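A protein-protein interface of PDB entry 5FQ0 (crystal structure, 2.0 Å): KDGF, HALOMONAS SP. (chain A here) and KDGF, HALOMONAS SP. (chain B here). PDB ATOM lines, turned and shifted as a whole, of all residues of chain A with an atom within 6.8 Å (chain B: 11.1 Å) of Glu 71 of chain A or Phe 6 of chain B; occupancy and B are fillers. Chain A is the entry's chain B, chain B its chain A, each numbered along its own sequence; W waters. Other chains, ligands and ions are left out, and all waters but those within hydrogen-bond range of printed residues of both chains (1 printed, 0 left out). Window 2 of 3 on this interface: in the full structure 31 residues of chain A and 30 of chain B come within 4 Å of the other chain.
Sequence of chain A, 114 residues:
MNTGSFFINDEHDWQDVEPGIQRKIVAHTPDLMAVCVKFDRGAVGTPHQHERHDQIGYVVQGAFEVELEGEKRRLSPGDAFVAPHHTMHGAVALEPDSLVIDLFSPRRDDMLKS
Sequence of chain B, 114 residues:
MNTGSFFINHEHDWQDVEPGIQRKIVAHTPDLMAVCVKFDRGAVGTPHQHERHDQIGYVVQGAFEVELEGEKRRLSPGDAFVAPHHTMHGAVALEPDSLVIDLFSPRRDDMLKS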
ATOM      1  N   GLU A  65      -7.139  21.377  35.903  1.00  0.00           N
ATOM      2  CA  GLU A  65      -5.749  20.982  36.082  1.00  0.00           C
ATOM      3  C   GLU A  65      -5.391  20.082  34.911  1.00  0.00           C
ATOM      4  O   GLU A  65      -6.019  19.034  34.694  1.00  0.00           O
ATOM      5  CB  GLU A  65      -5.447  20.277  37.397  1.00  0.00           C
ATOM      6  CG  GLU A  65      -4.043  19.683  37.278  1.00  0.00           C
ATOM      7  CD  GLU A  65      -3.369  19.279  38.571  1.00  0.00           C
ATOM      8  OE1 GLU A  65      -2.809  20.171  39.254  1.00  0.00           O
ATOM      9  OE2 GLU A  65      -3.340  18.065  38.866  1.00  0.00           O
ATOM     10  N   VAL A  66      -4.406  20.498  34.140  1.00  0.00           N
ATOM     11  CA  VAL A  66      -4.029  19.757  32.944  1.00  0.00           C
ATOM     12  C   VAL A  66      -2.681  19.105  33.213  1.00  0.00           C
ATOM     13  O   VAL A  66      -1.763  19.739  33.785  1.00  0.00           O
ATOM     14  CB  VAL A  66      -3.963  20.665  31.698  1.00  0.00           C
ATOM     15  CG1 VAL A  66      -3.220  19.970  30.555  1.00  0.00           C
ATOM     16  CG2 VAL A  66      -5.374  21.058  31.250  1.00  0.00           C
ATOM     17  N   GLU A  67      -2.591  17.845  32.810  1.00  0.00           N
ATOM     18  CA  GLU A  67      -1.363  17.074  32.899  1.00  0.00           C
ATOM     19  C   GLU A  67      -0.775  16.841  31.520  1.00  0.00           C
ATOM     20  O   GLU A  67      -1.453  16.303  30.637  1.00  0.00           O
ATOM     21  CB  GLU A  67      -1.635  15.735  33.574  1.00  0.00           C
ATOM     22  CG  GLU A  67      -0.393  14.878  33.673  1.00  0.00           C
ATOM     23  CD  GLU A  67      -0.671  13.528  34.303  1.00  0.00           C
ATOM     24  OE1 GLU A  67      -1.816  13.028  34.214  1.00  0.00           O
ATOM     25  OE2 GLU A  67       0.275  12.979  34.897  1.00  0.00           O
ATOM     26  N   LEU A  68       0.484  17.254  31.349  1.00  0.00           N
ATOM     27  CA  LEU A  68       1.201  17.111  30.105  1.00  0.00           C
ATOM     28  C   LEU A  68       2.492  16.364  30.391  1.00  0.00           C
ATOM     29  O   LEU A  68       3.392  16.919  31.014  1.00  0.00           O
ATOM     30  CB  LEU A  68       1.580  18.479  29.561  1.00  0.00           C
ATOM     31  CG  LEU A  68       0.805  19.194  28.476  1.00  0.00           C
ATOM     32  CD1 LEU A  68       1.703  20.349  28.018  1.00  0.00           C
ATOM     33  CD2 LEU A  68       0.451  18.232  27.335  1.00  0.00           C
ATOM     34  N   GLU A  69       2.569  15.128  29.918  1.00  0.00           N
ATOM     35  CA  GLU A  69       3.691  14.207  30.192  1.00  0.00           C
ATOM     36  C   GLU A  69       4.129  14.332  31.657  1.00  0.00           C
ATOM     37  O   GLU A  69       5.263  14.717  31.937  1.00  0.00           O
ATOM     38  CB  GLU A  69       4.874  14.453  29.232  1.00  0.00           C
ATOM     39  CG  GLU A  69       4.703  13.921  27.805  1.00  0.00           C
ATOM     40  CD  GLU A  69       4.607  12.397  27.689  1.00  0.00           C
ATOM     41  OE1 GLU A  69       4.869  11.694  28.705  1.00  0.00           O
ATOM     42  OE2 GLU A  69       4.275  11.890  26.586  1.00  0.00           O
ATOM     43  N   GLY A  70       3.205  14.073  32.580  1.00  0.00           N
ATOM     44  CA  GLY A  70       3.496  14.181  34.019  1.00  0.00           C
ATOM     45  C   GLY A  70       3.566  15.566  34.654  1.00  0.00           C
ATOM     46  O   GLY A  70       3.380  15.674  35.858  1.00  0.00           O
ATOM     47  N   GLU A  71       3.829  16.622  33.877  1.00  0.00           N
ATOM     48  CA  GLU A  71       3.777  18.003  34.391  1.00  0.00           C
ATOM     49  C   GLU A  71       2.313  18.519  34.522  1.00  0.00           C
ATOM     50  O   GLU A  71       1.533  18.431  33.576  1.00  0.00           O
ATOM     51  CB  GLU A  71       4.622  18.960  33.515  1.00  0.00           C
ATOM     52  CG  GLU A  71       4.686  20.401  34.049  1.00  0.00           C
ATOM     53  CD  GLU A  71       5.254  21.444  33.069  1.00  0.00           C
ATOM     54  OE1 GLU A  71       5.675  21.082  31.948  1.00  0.00           O
ATOM     55  OE2 GLU A  71       5.276  22.648  33.409  1.00  0.00           O
ATOM     56  N   LYS A  72       1.959  19.067  35.681  1.00  0.00           N
ATOM     57  CA  LYS A  72       0.611  19.594  35.939  1.00  0.00           C
ATOM     58  C   LYS A  72       0.603  21.122  36.015  1.00  0.00           C
ATOM     59  O   LYS A  72       1.496  21.729  36.639  1.00  0.00           O
ATOM     60  CB  LYS A  72       0.031  19.083  37.258  1.00  0.00           C
ATOM     61  CG  LYS A  72       0.221  17.608  37.572  1.00  0.00           C
ATOM     62  CD  LYS A  72      -0.763  16.716  36.852  1.00  0.00           C
ATOM     63  CE  LYS A  72      -0.581  15.259  37.256  1.00  0.00           C
ATOM     64  NZ  LYS A  72      -1.250  14.941  38.542  1.00  0.00           N
ATOM     65  N   ARG A  73      -0.414  21.746  35.412  1.00  0.00           N
ATOM     66  CA  ARG A  73      -0.679  23.177  35.628  1.00  0.00           C
ATOM     67  C   ARG A  73      -2.172  23.450  35.765  1.00  0.00           C
ATOM     68  O   ARG A  73      -2.990  22.752  35.144  1.00  0.00           O
ATOM     69  CB  ARG A  73      -0.136  24.024  34.474  1.00  0.00           C
ATOM     70  CG  ARG A  73       1.339  23.831  34.194  1.00  0.00           C
ATOM     71  CD  ARG A  73       2.190  24.678  35.115  1.00  0.00           C
ATOM     72  NE  ARG A  73       2.452  25.960  34.494  1.00  0.00           N
ATOM     73  CZ  ARG A  73       3.416  26.164  33.599  1.00  0.00           C
ATOM     74  NH1 ARG A  73       4.219  25.161  33.238  1.00  0.00           N
ATOM     75  NH2 ARG A  73       3.579  27.373  33.070  1.00  0.00           N
ATOM     76  N   ARG A  74      -2.515  24.478  36.542  1.00  0.00           N
ATOM     77  CA  ARG A  74      -3.909  24.947  36.682  1.00  0.00           C
ATOM     78  C   ARG A  74      -4.112  25.980  35.585  1.00  0.00           C
ATOM     79  O   ARG A  74      -3.404  26.975  35.547  1.00  0.00           O
ATOM     80  CB  ARG A  74      -4.162  25.576  38.061  1.00  0.00           C
ATOM     81  CG  ARG A  74      -5.531  26.263  38.250  1.00  0.00           C
ATOM     82  CD  ARG A  74      -5.625  27.143  39.529  1.00  0.00           C
ATOM     83  NE  ARG A  74      -4.938  26.517  40.674  1.00  0.00           N
ATOM     84  CZ  ARG A  74      -3.803  26.947  41.239  1.00  0.00           C
ATOM     85  NH1 ARG A  74      -3.218  28.071  40.849  1.00  0.00           N
ATOM     86  NH2 ARG A  74      -3.261  26.250  42.228  1.00  0.00           N
ATOM     87  N   LEU A  75      -5.065  25.739  34.695  1.00  0.00           N
ATOM     88  CA  LEU A  75      -5.300  26.624  33.530  1.00  0.00           C
ATOM     89  C   LEU A  75      -6.671  27.263  33.655  1.00  0.00           C
ATOM     90  O   LEU A  75      -7.662  26.579  33.936  1.00  0.00           O
ATOM     91  CB  LEU A  75      -5.220  25.831  32.212  1.00  0.00           C
ATOM     92  CG  LEU A  75      -3.902  25.112  31.876  1.00  0.00           C
ATOM     93  CD1 LEU A  75      -3.983  24.574  30.462  1.00  0.00           C
ATOM     94  CD2 LEU A  75      -2.653  25.992  32.009  1.00  0.00           C
ATOM     95  N   ASP A  79      -5.892  30.574  28.983  1.00  0.00           N
ATOM     96  CA  ASP A  79      -4.700  29.723  28.981  1.00  0.00           C
ATOM     97  C   ASP A  79      -4.866  28.535  28.071  1.00  0.00           C
ATOM     98  O   ASP A  79      -6.006  28.166  27.723  1.00  0.00           O
ATOM     99  CB  ASP A  79      -4.342  29.207  30.394  1.00  0.00           C
ATOM    100  CG  ASP A  79      -4.096  30.329  31.415  1.00  0.00           C
ATOM    101  OD1 ASP A  79      -3.671  31.457  31.077  1.00  0.00           O
ATOM    102  OD2 ASP A  79      -4.335  30.046  32.602  1.00  0.00           O
ATOM    103  N   ALA A  80      -3.753  27.893  27.700  1.00  0.00           N
ATOM    104  CA  ALA A  80      -3.836  26.726  26.808  1.00  0.00           C
ATOM    105  C   ALA A  80      -2.742  25.672  27.043  1.00  0.00           C
ATOM    106  O   ALA A  80      -1.724  25.955  27.674  1.00  0.00           O
ATOM    107  CB  ALA A  80      -3.833  27.180  25.346  1.00  0.00           C
ATOM    108  N   PHE A  81      -2.942  24.463  26.541  1.00  0.00           N
ATOM    109  CA  PHE A  81      -1.814  23.515  26.375  1.00  0.00           C
ATOM    110  C   PHE A  81      -1.713  23.059  24.923  1.00  0.00           C
ATOM    111  O   PHE A  81      -2.736  23.052  24.209  1.00  0.00           O
ATOM    112  CB  PHE A  81      -1.943  22.286  27.292  1.00  0.00           C
ATOM    113  CG  PHE A  81      -3.052  21.341  26.917  1.00  0.00           C
ATOM    114  CD1 PHE A  81      -4.366  21.568  27.349  1.00  0.00           C
ATOM    115  CD2 PHE A  81      -2.787  20.208  26.158  1.00  0.00           C
ATOM    116  CE1 PHE A  81      -5.380  20.701  27.017  1.00  0.00           C
ATOM    117  CE2 PHE A  81      -3.804  19.313  25.825  1.00  0.00           C
ATOM    118  CZ  PHE A  81      -5.104  19.557  26.247  1.00  0.00           C
ATOM    119  N   VAL A  82      -0.508  22.642  24.505  1.00  0.00           N
ATOM    120  CA  VAL A  82      -0.315  21.973  23.220  1.00  0.00           C
ATOM    121  C   VAL A  82       0.262  20.600  23.501  1.00  0.00           C
ATOM    122  O   VAL A  82       1.244  20.517  24.218  1.00  0.00           O
ATOM    123  CB  VAL A  82       0.492  22.829  22.177  1.00  0.00           C
ATOM    124  CG1 VAL A  82       1.829  23.337  22.738  1.00  0.00           C
ATOM    125  CG2 VAL A  82       0.689  22.099  20.834  1.00  0.00           C
ATOM    126  N   THR B   3       7.215  18.008  21.895  1.00  0.00           N
ATOM    127  CA  THR B   3       7.291  17.707  23.365  1.00  0.00           C
ATOM    128  C   THR B   3       6.088  18.092  24.280  1.00  0.00           C
ATOM    129  O   THR B   3       5.831  17.403  25.279  1.00  0.00           O
ATOM    130  CB  THR B   3       8.587  18.258  24.013  1.00  0.00           C
ATOM    131  OG1 THR B   3       8.596  17.875  25.392  1.00  0.00           O
ATOM    132  CG2 THR B   3       8.697  19.803  23.907  1.00  0.00           C
ATOM    133  N   GLY B   4       5.401  19.197  23.985  1.00  0.00           N
ATOM    134  CA  GLY B   4       4.327  19.677  24.885  1.00  0.00           C
ATOM    135  C   GLY B   4       4.675  20.966  25.632  1.00  0.00           C
ATOM    136  O   GLY B   4       5.782  21.102  26.138  1.00  0.00           O
ATOM    137  N   SER B   5       3.752  21.931  25.647  1.00  0.00           N
ATOM    138  CA  SER B   5       3.943  23.216  26.349  1.00  0.00           C
ATOM    139  C   SER B   5       2.627  23.696  26.920  1.00  0.00           C
ATOM    140  O   SER B   5       1.543  23.242  26.505  1.00  0.00           O
ATOM    141  CB  SER B   5       4.462  24.336  25.423  1.00  0.00           C
ATOM    142  OG  SER B   5       5.437  23.860  24.548  1.00  0.00           O
ATOM    143  N   PHE B   6       2.736  24.655  27.827  1.00  0.00           N
ATOM    144  CA  PHE B   6       1.582  25.363  28.371  1.00  0.00           C
ATOM    145  C   PHE B   6       1.639  26.801  27.862  1.00  0.00           C
ATOM    146  O   PHE B   6       2.728  27.330  27.612  1.00  0.00           O
ATOM    147  CB  PHE B   6       1.628  25.317  29.892  1.00  0.00           C
ATOM    148  CG  PHE B   6       1.348  23.942  30.470  1.00  0.00           C
ATOM    149  CD1 PHE B   6       0.025  23.468  30.584  1.00  0.00           C
ATOM    150  CD2 PHE B   6       2.400  23.120  30.921  1.00  0.00           C
ATOM    151  CE1 PHE B   6      -0.240  22.213  31.102  1.00  0.00           C
ATOM    152  CE2 PHE B   6       2.128  21.855  31.429  1.00  0.00           C
ATOM    153  CZ  PHE B   6       0.813  21.414  31.545  1.00  0.00           C
ATOM    154  N   PHE B   7       0.482  27.431  27.695  1.00  0.00           N
ATOM    155  CA  PHE B   7       0.418  28.869  27.411  1.00  0.00           C
ATOM    156  C   PHE B   7      -0.326  29.535  28.571  1.00  0.00           C
ATOM    157  O   PHE B   7      -1.510  29.276  28.778  1.00  0.00           O
ATOM    158  CB  PHE B   7      -0.344  29.119  26.118  1.00  0.00           C
ATOM    159  CG  PHE B   7      -0.496  30.572  25.777  1.00  0.00           C
ATOM    160  CD1 PHE B   7       0.593  31.299  25.319  1.00  0.00           C
ATOM    161  CD2 PHE B   7      -1.723  31.227  25.960  1.00  0.00           C
ATOM    162  CE1 PHE B   7       0.452  32.650  24.992  1.00  0.00           C
ATOM    163  CE2 PHE B   7      -1.861  32.572  25.645  1.00  0.00           C
ATOM    164  CZ  PHE B   7      -0.776  33.275  25.162  1.00  0.00           C
ATOM    165  N   ILE B   8       0.364  30.379  29.338  1.00  0.00           N
ATOM    166  CA  ILE B   8      -0.285  31.144  30.411  1.00  0.00           C
ATOM    167  C   ILE B   8      -0.519  32.557  29.898  1.00  0.00           C
ATOM    168  O   ILE B   8       0.419  33.355  29.754  1.00  0.00           O
ATOM    169  CB  ILE B   8       0.529  31.185  31.724  1.00  0.00           C
ATOM    170  CG1 ILE B   8       1.020  29.783  32.130  1.00  0.00           C
ATOM    171  CG2 ILE B   8      -0.319  31.820  32.840  1.00  0.00           C
ATOM    172  CD1 ILE B   8      -0.108  28.758  32.267  1.00  0.00           C
ATOM    173  N   ASN B   9      -1.780  32.853  29.585  1.00  0.00           N
ATOM    174  CA  ASN B   9      -2.127  34.089  28.874  1.00  0.00           C
ATOM    175  C   ASN B   9      -1.541  35.363  29.525  1.00  0.00           C
ATOM    176  O   ASN B   9      -0.992  36.238  28.840  1.00  0.00           O
ATOM    177  CB  ASN B   9      -3.650  34.222  28.776  1.00  0.00           C
ATOM    178  CG  ASN B   9      -4.066  35.491  28.052  1.00  0.00           C
ATOM    179  OD1 ASN B   9      -3.552  35.788  26.989  1.00  0.00           O
ATOM    180  ND2 ASN B   9      -4.966  36.272  28.654  1.00  0.00           N
ATOM    181  N   HIS B  10      -1.679  35.456  30.849  1.00  0.00           N
ATOM    182  CA  HIS B  10      -1.198  36.618  31.632  1.00  0.00           C
ATOM    183  C   HIS B  10       0.284  36.939  31.477  1.00  0.00           C
ATOM    184  O   HIS B  10       0.707  38.086  31.676  1.00  0.00           O
ATOM    185  CB  HIS B  10      -1.496  36.411  33.117  1.00  0.00           C
ATOM    186  CG  HIS B  10      -2.905  36.725  33.468  1.00  0.00           C
ATOM    187  ND1 HIS B  10      -3.517  36.251  34.609  1.00  0.00           N
ATOM    188  CD2 HIS B  10      -3.841  37.447  32.806  1.00  0.00           C
ATOM    189  CE1 HIS B  10      -4.767  36.682  34.645  1.00  0.00           C
ATOM    190  NE2 HIS B  10      -4.987  37.414  33.565  1.00  0.00           N
ATOM    191  N   GLU B  11       1.048  35.902  31.162  1.00  0.00           N
ATOM    192  CA  GLU B  11       2.504  35.924  31.015  1.00  0.00           C
ATOM    193  C   GLU B  11       2.998  36.453  29.681  1.00  0.00           C
ATOM    194  O   GLU B  11       4.223  36.514  29.501  1.00  0.00           O
ATOM    195  CB  GLU B  11       3.038  34.488  31.066  1.00  0.00           C
ATOM    196  CG  GLU B  11       3.900  34.092  32.241  1.00  0.00           C
ATOM    197  CD  GLU B  11       3.071  33.760  33.441  1.00  0.00           C
ATOM    198  OE1 GLU B  11       2.191  34.581  33.739  1.00  0.00           O
ATOM    199  OE2 GLU B  11       3.300  32.710  34.071  1.00  0.00           O
ATOM    200  N   HIS B  12       2.094  36.775  28.742  1.00  0.00           N
ATOM    201  CA  HIS B  12       2.523  37.173  27.383  1.00  0.00           C
ATOM    202  C   HIS B  12       1.892  38.518  26.998  1.00  0.00           C
ATOM    203  O   HIS B  12       0.725  38.746  27.293  1.00  0.00           O
ATOM    204  CB  HIS B  12       2.186  36.067  26.358  1.00  0.00           C
ATOM    205  CG  HIS B  12       2.760  34.718  26.707  1.00  0.00           C
ATOM    206  ND1 HIS B  12       3.847  34.178  26.049  1.00  0.00           N
ATOM    207  CD2 HIS B  12       2.411  33.812  27.655  1.00  0.00           C
ATOM    208  CE1 HIS B  12       4.136  32.996  26.567  1.00  0.00           C
ATOM    209  NE2 HIS B  12       3.283  32.753  27.548  1.00  0.00           N
ATOM    210  N   ILE B  25       0.600  34.780  19.929  1.00  0.00           N
ATOM    211  CA  ILE B  25       0.710  33.400  19.458  1.00  0.00           C
ATOM    212  C   ILE B  25       0.473  32.502  20.668  1.00  0.00           C
ATOM    213  O   ILE B  25       1.150  32.628  21.679  1.00  0.00           O
ATOM    214  CB  ILE B  25       2.079  33.093  18.826  1.00  0.00           C
ATOM    215  CG1 ILE B  25       2.419  34.071  17.671  1.00  0.00           C
ATOM    216  CG2 ILE B  25       2.136  31.638  18.399  1.00  0.00           C
ATOM    217  CD1 ILE B  25       1.370  34.188  16.572  1.00  0.00           C
ATOM    218  N   VAL B  26      -0.500  31.606  20.587  1.00  0.00           N
ATOM    219  CA  VAL B  26      -0.835  30.787  21.742  1.00  0.00           C
ATOM    220  C   VAL B  26       0.016  29.483  21.771  1.00  0.00           C
ATOM    221  O   VAL B  26       0.693  29.192  22.755  1.00  0.00           O
ATOM    222  CB  VAL B  26      -2.357  30.438  21.751  1.00  0.00           C
ATOM    223  CG1 VAL B  26      -2.668  29.380  22.790  1.00  0.00           C
ATOM    224  CG2 VAL B  26      -3.249  31.670  21.945  1.00  0.00           C
ATOM    225  N   ALA B  27      -0.068  28.661  20.736  1.00  0.00           N
ATOM    226  CA  ALA B  27       0.710  27.416  20.715  1.00  0.00           C
ATOM    227  C   ALA B  27       0.826  26.977  19.288  1.00  0.00           C
ATOM    228  O   ALA B  27       0.071  27.455  18.419  1.00  0.00           O
ATOM    229  CB  ALA B  27       0.043  26.333  21.547  1.00  0.00           C
ATOM    230  N   HIS B  28       1.773  26.099  19.010  1.00  0.00           N
ATOM    231  CA  HIS B  28       1.842  25.498  17.677  1.00  0.00           C
ATOM    232  C   HIS B  28       2.693  24.249  17.623  1.00  0.00           C
ATOM    233  O   HIS B  28       3.575  24.047  18.446  1.00  0.00           O
ATOM    234  CB  HIS B  28       2.354  26.484  16.637  1.00  0.00           C
ATOM    235  CG  HIS B  28       3.684  27.064  16.980  1.00  0.00           C
ATOM    236  ND1 HIS B  28       4.866  26.513  16.538  1.00  0.00           N
ATOM    237  CD2 HIS B  28       4.021  28.150  17.718  1.00  0.00           C
ATOM    238  CE1 HIS B  28       5.879  27.225  17.003  1.00  0.00           C
ATOM    239  NE2 HIS B  28       5.392  28.232  17.710  1.00  0.00           N
ATOM    240  N   THR B  29       2.382  23.413  16.643  1.00  0.00           N
ATOM    241  CA  THR B  29       3.234  22.326  16.201  1.00  0.00           C
ATOM    242  C   THR B  29       3.421  22.621  14.715  1.00  0.00           C
ATOM    243  O   THR B  29       2.857  23.603  14.214  1.00  0.00           O
ATOM    244  CB  THR B  29       2.525  20.970  16.317  1.00  0.00           C
ATOM    245  OG1 THR B  29       1.440  20.922  15.367  1.00  0.00           O
ATOM    246  CG2 THR B  29       1.968  20.761  17.704  1.00  0.00           C
ATOM    247  N   ALA B  34      -2.548  28.012  17.098  1.00  0.00           N
ATOM    248  CA  ALA B  34      -3.615  28.878  17.655  1.00  0.00           C
ATOM    249  C   ALA B  34      -3.025  30.225  17.936  1.00  0.00           C
ATOM    250  O   ALA B  34      -1.891  30.318  18.424  1.00  0.00           O
ATOM    251  CB  ALA B  34      -4.247  28.296  18.925  1.00  0.00           C
HETATM  252  O   HOH W   1      -3.420  33.669  32.450  1.00  0.00           O
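The backbone carbonyl oxygen of Ala 34 of chain B sits at hydrogen-bond distance from the backbone NH of Val 26 of chain B, at 2.9 Å.
N of Ala 34 of chain B is in hydrogen-bond range of O of Ala 27 of chain B (3.0 Å).
The backbone NH (N) of Val 66 of chain A lies within hydrogen-bond range of the backbone carbonyl oxygen (O) of Arg 73 of chain A.
The side-chain carboxylate (OE2) of Glu 71 of chain A is in salt-bridge range of the guanidinium group (NH1) of Arg 73 of chain A, at 2.7 Å.
Phe 6 of chain B touches Val 66 of chain A.
C of Gly 4 of chain B touches CD1 of Leu 68 of chain A, 3.9 Å away.
Ser 5 of chain B touches Leu 68 of chain A (O to CD1, 3.3 Å).
Phe 6 of chain B touches Leu 68 of chain A.
Phe 6 of chain B touches Arg 73 of chain A.
Ile 8 of chain B touches Arg 73 of chain A (CG1 to NH2, 3.6 Å).
Phe 6 of chain B touches Leu 75 of chain A (CD1 to CD2, 3.9 Å).
CD2 of Leu 75 of chain A touches CD1 of Ile 8 of chain B, at 3.8 Å.
Asp 79 of chain A touches Phe 7 of chain B (CA to O, 3.2 Å).
Asp 79 of chain A touches Ile 8 of chain B (OD1 to CA, 3.5 Å).
The backbone carbonyl oxygen (O) of Ser 5 of chain B lies within hydrogen-bond range of the backbone NH (N) of Val 82 of chain A (2.9 Å).
The backbone NH (N) of Phe 7 of chain B sits at hydrogen-bond distance from the backbone carbonyl oxygen (O) of Ala 80 of chain A (2.7 Å).
The backbone NH (N) of Asn 9 of chain B lies within hydrogen-bond range of the side-chain carboxylate (OD1) of Asp 79 of chain A (2.8 Å).
Water W1 lies within hydrogen-bond range of OD1 of Asp 79 of chain A (2.6 Å), N of His 10 of chain B (3.0 Å) and N of Asn 9 of chain B (3.4 Å).
Along chain B the printed residues that touch a printed residue of chain A span positions 4 to 29.
Among the printed residues, no Asp or Glu carboxylate lies within 4 Å of a Lys or Arg side-chain nitrogen of the other chain.
Of chain B, only Phe 6 comes within 4 Å of Glu 71 of chain A.
Printed residues of chain A within 4 Å of Phe 6 of chain B: Val 66 (3.8 Å), Leu 68 (3.6 Å), Glu 71 (3.6 Å), Arg 73 (3.5 Å), Leu 75 (3.9 Å) and Ala 80 (3.4 Å).
Val 66 of chain A touches just one residue of chain B: Phe 6 (3.8 Å).
Glu 67 of chain A touches none of the printed residues of chain B.
No residue of chain B comes within 4 Å of Gly 70 of chain A.
No residue of chain B comes within 4 Å of Lys 72 of chain A.
Of the printed residues of chain B, Arg 73 of chain A touches Phe 6 and Ile 8.
Printed residues of chain B within 4 Å of Asp 79 of chain A: Phe 7, Ile 8 and Asn 9.
Printed residues of chain A within 4 Å of Ser 5 of chain B: Leu 68, Phe 81 and Val 82.
Of the printed residues of chain B, Leu 75 of chain A touches Phe 6 and Ile 8.
Printed residues of chain A within 4 Å of Gly 4 of chain B: Leu 68 (3.9 Å) and Val 82 (3.3 Å).
Of the printed residues of chain A, Asn 9 of chain B touches Asp 79 (2.8 Å).
Glu 65 of chain A touches none of the printed residues of chain B.
The nearest residue of chain B that does not touch Glu 71 of chain A is Gly 4 of chain B (5.8 Å).
The nearest printed residue of chain A that does not touch Phe 6 of chain B is Phe 81 of chain A (4.01 Å).
The nearest printed residue of chain B that does not touch Phe 81 of chain A is Phe 6 of chain B (4.01 Å).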
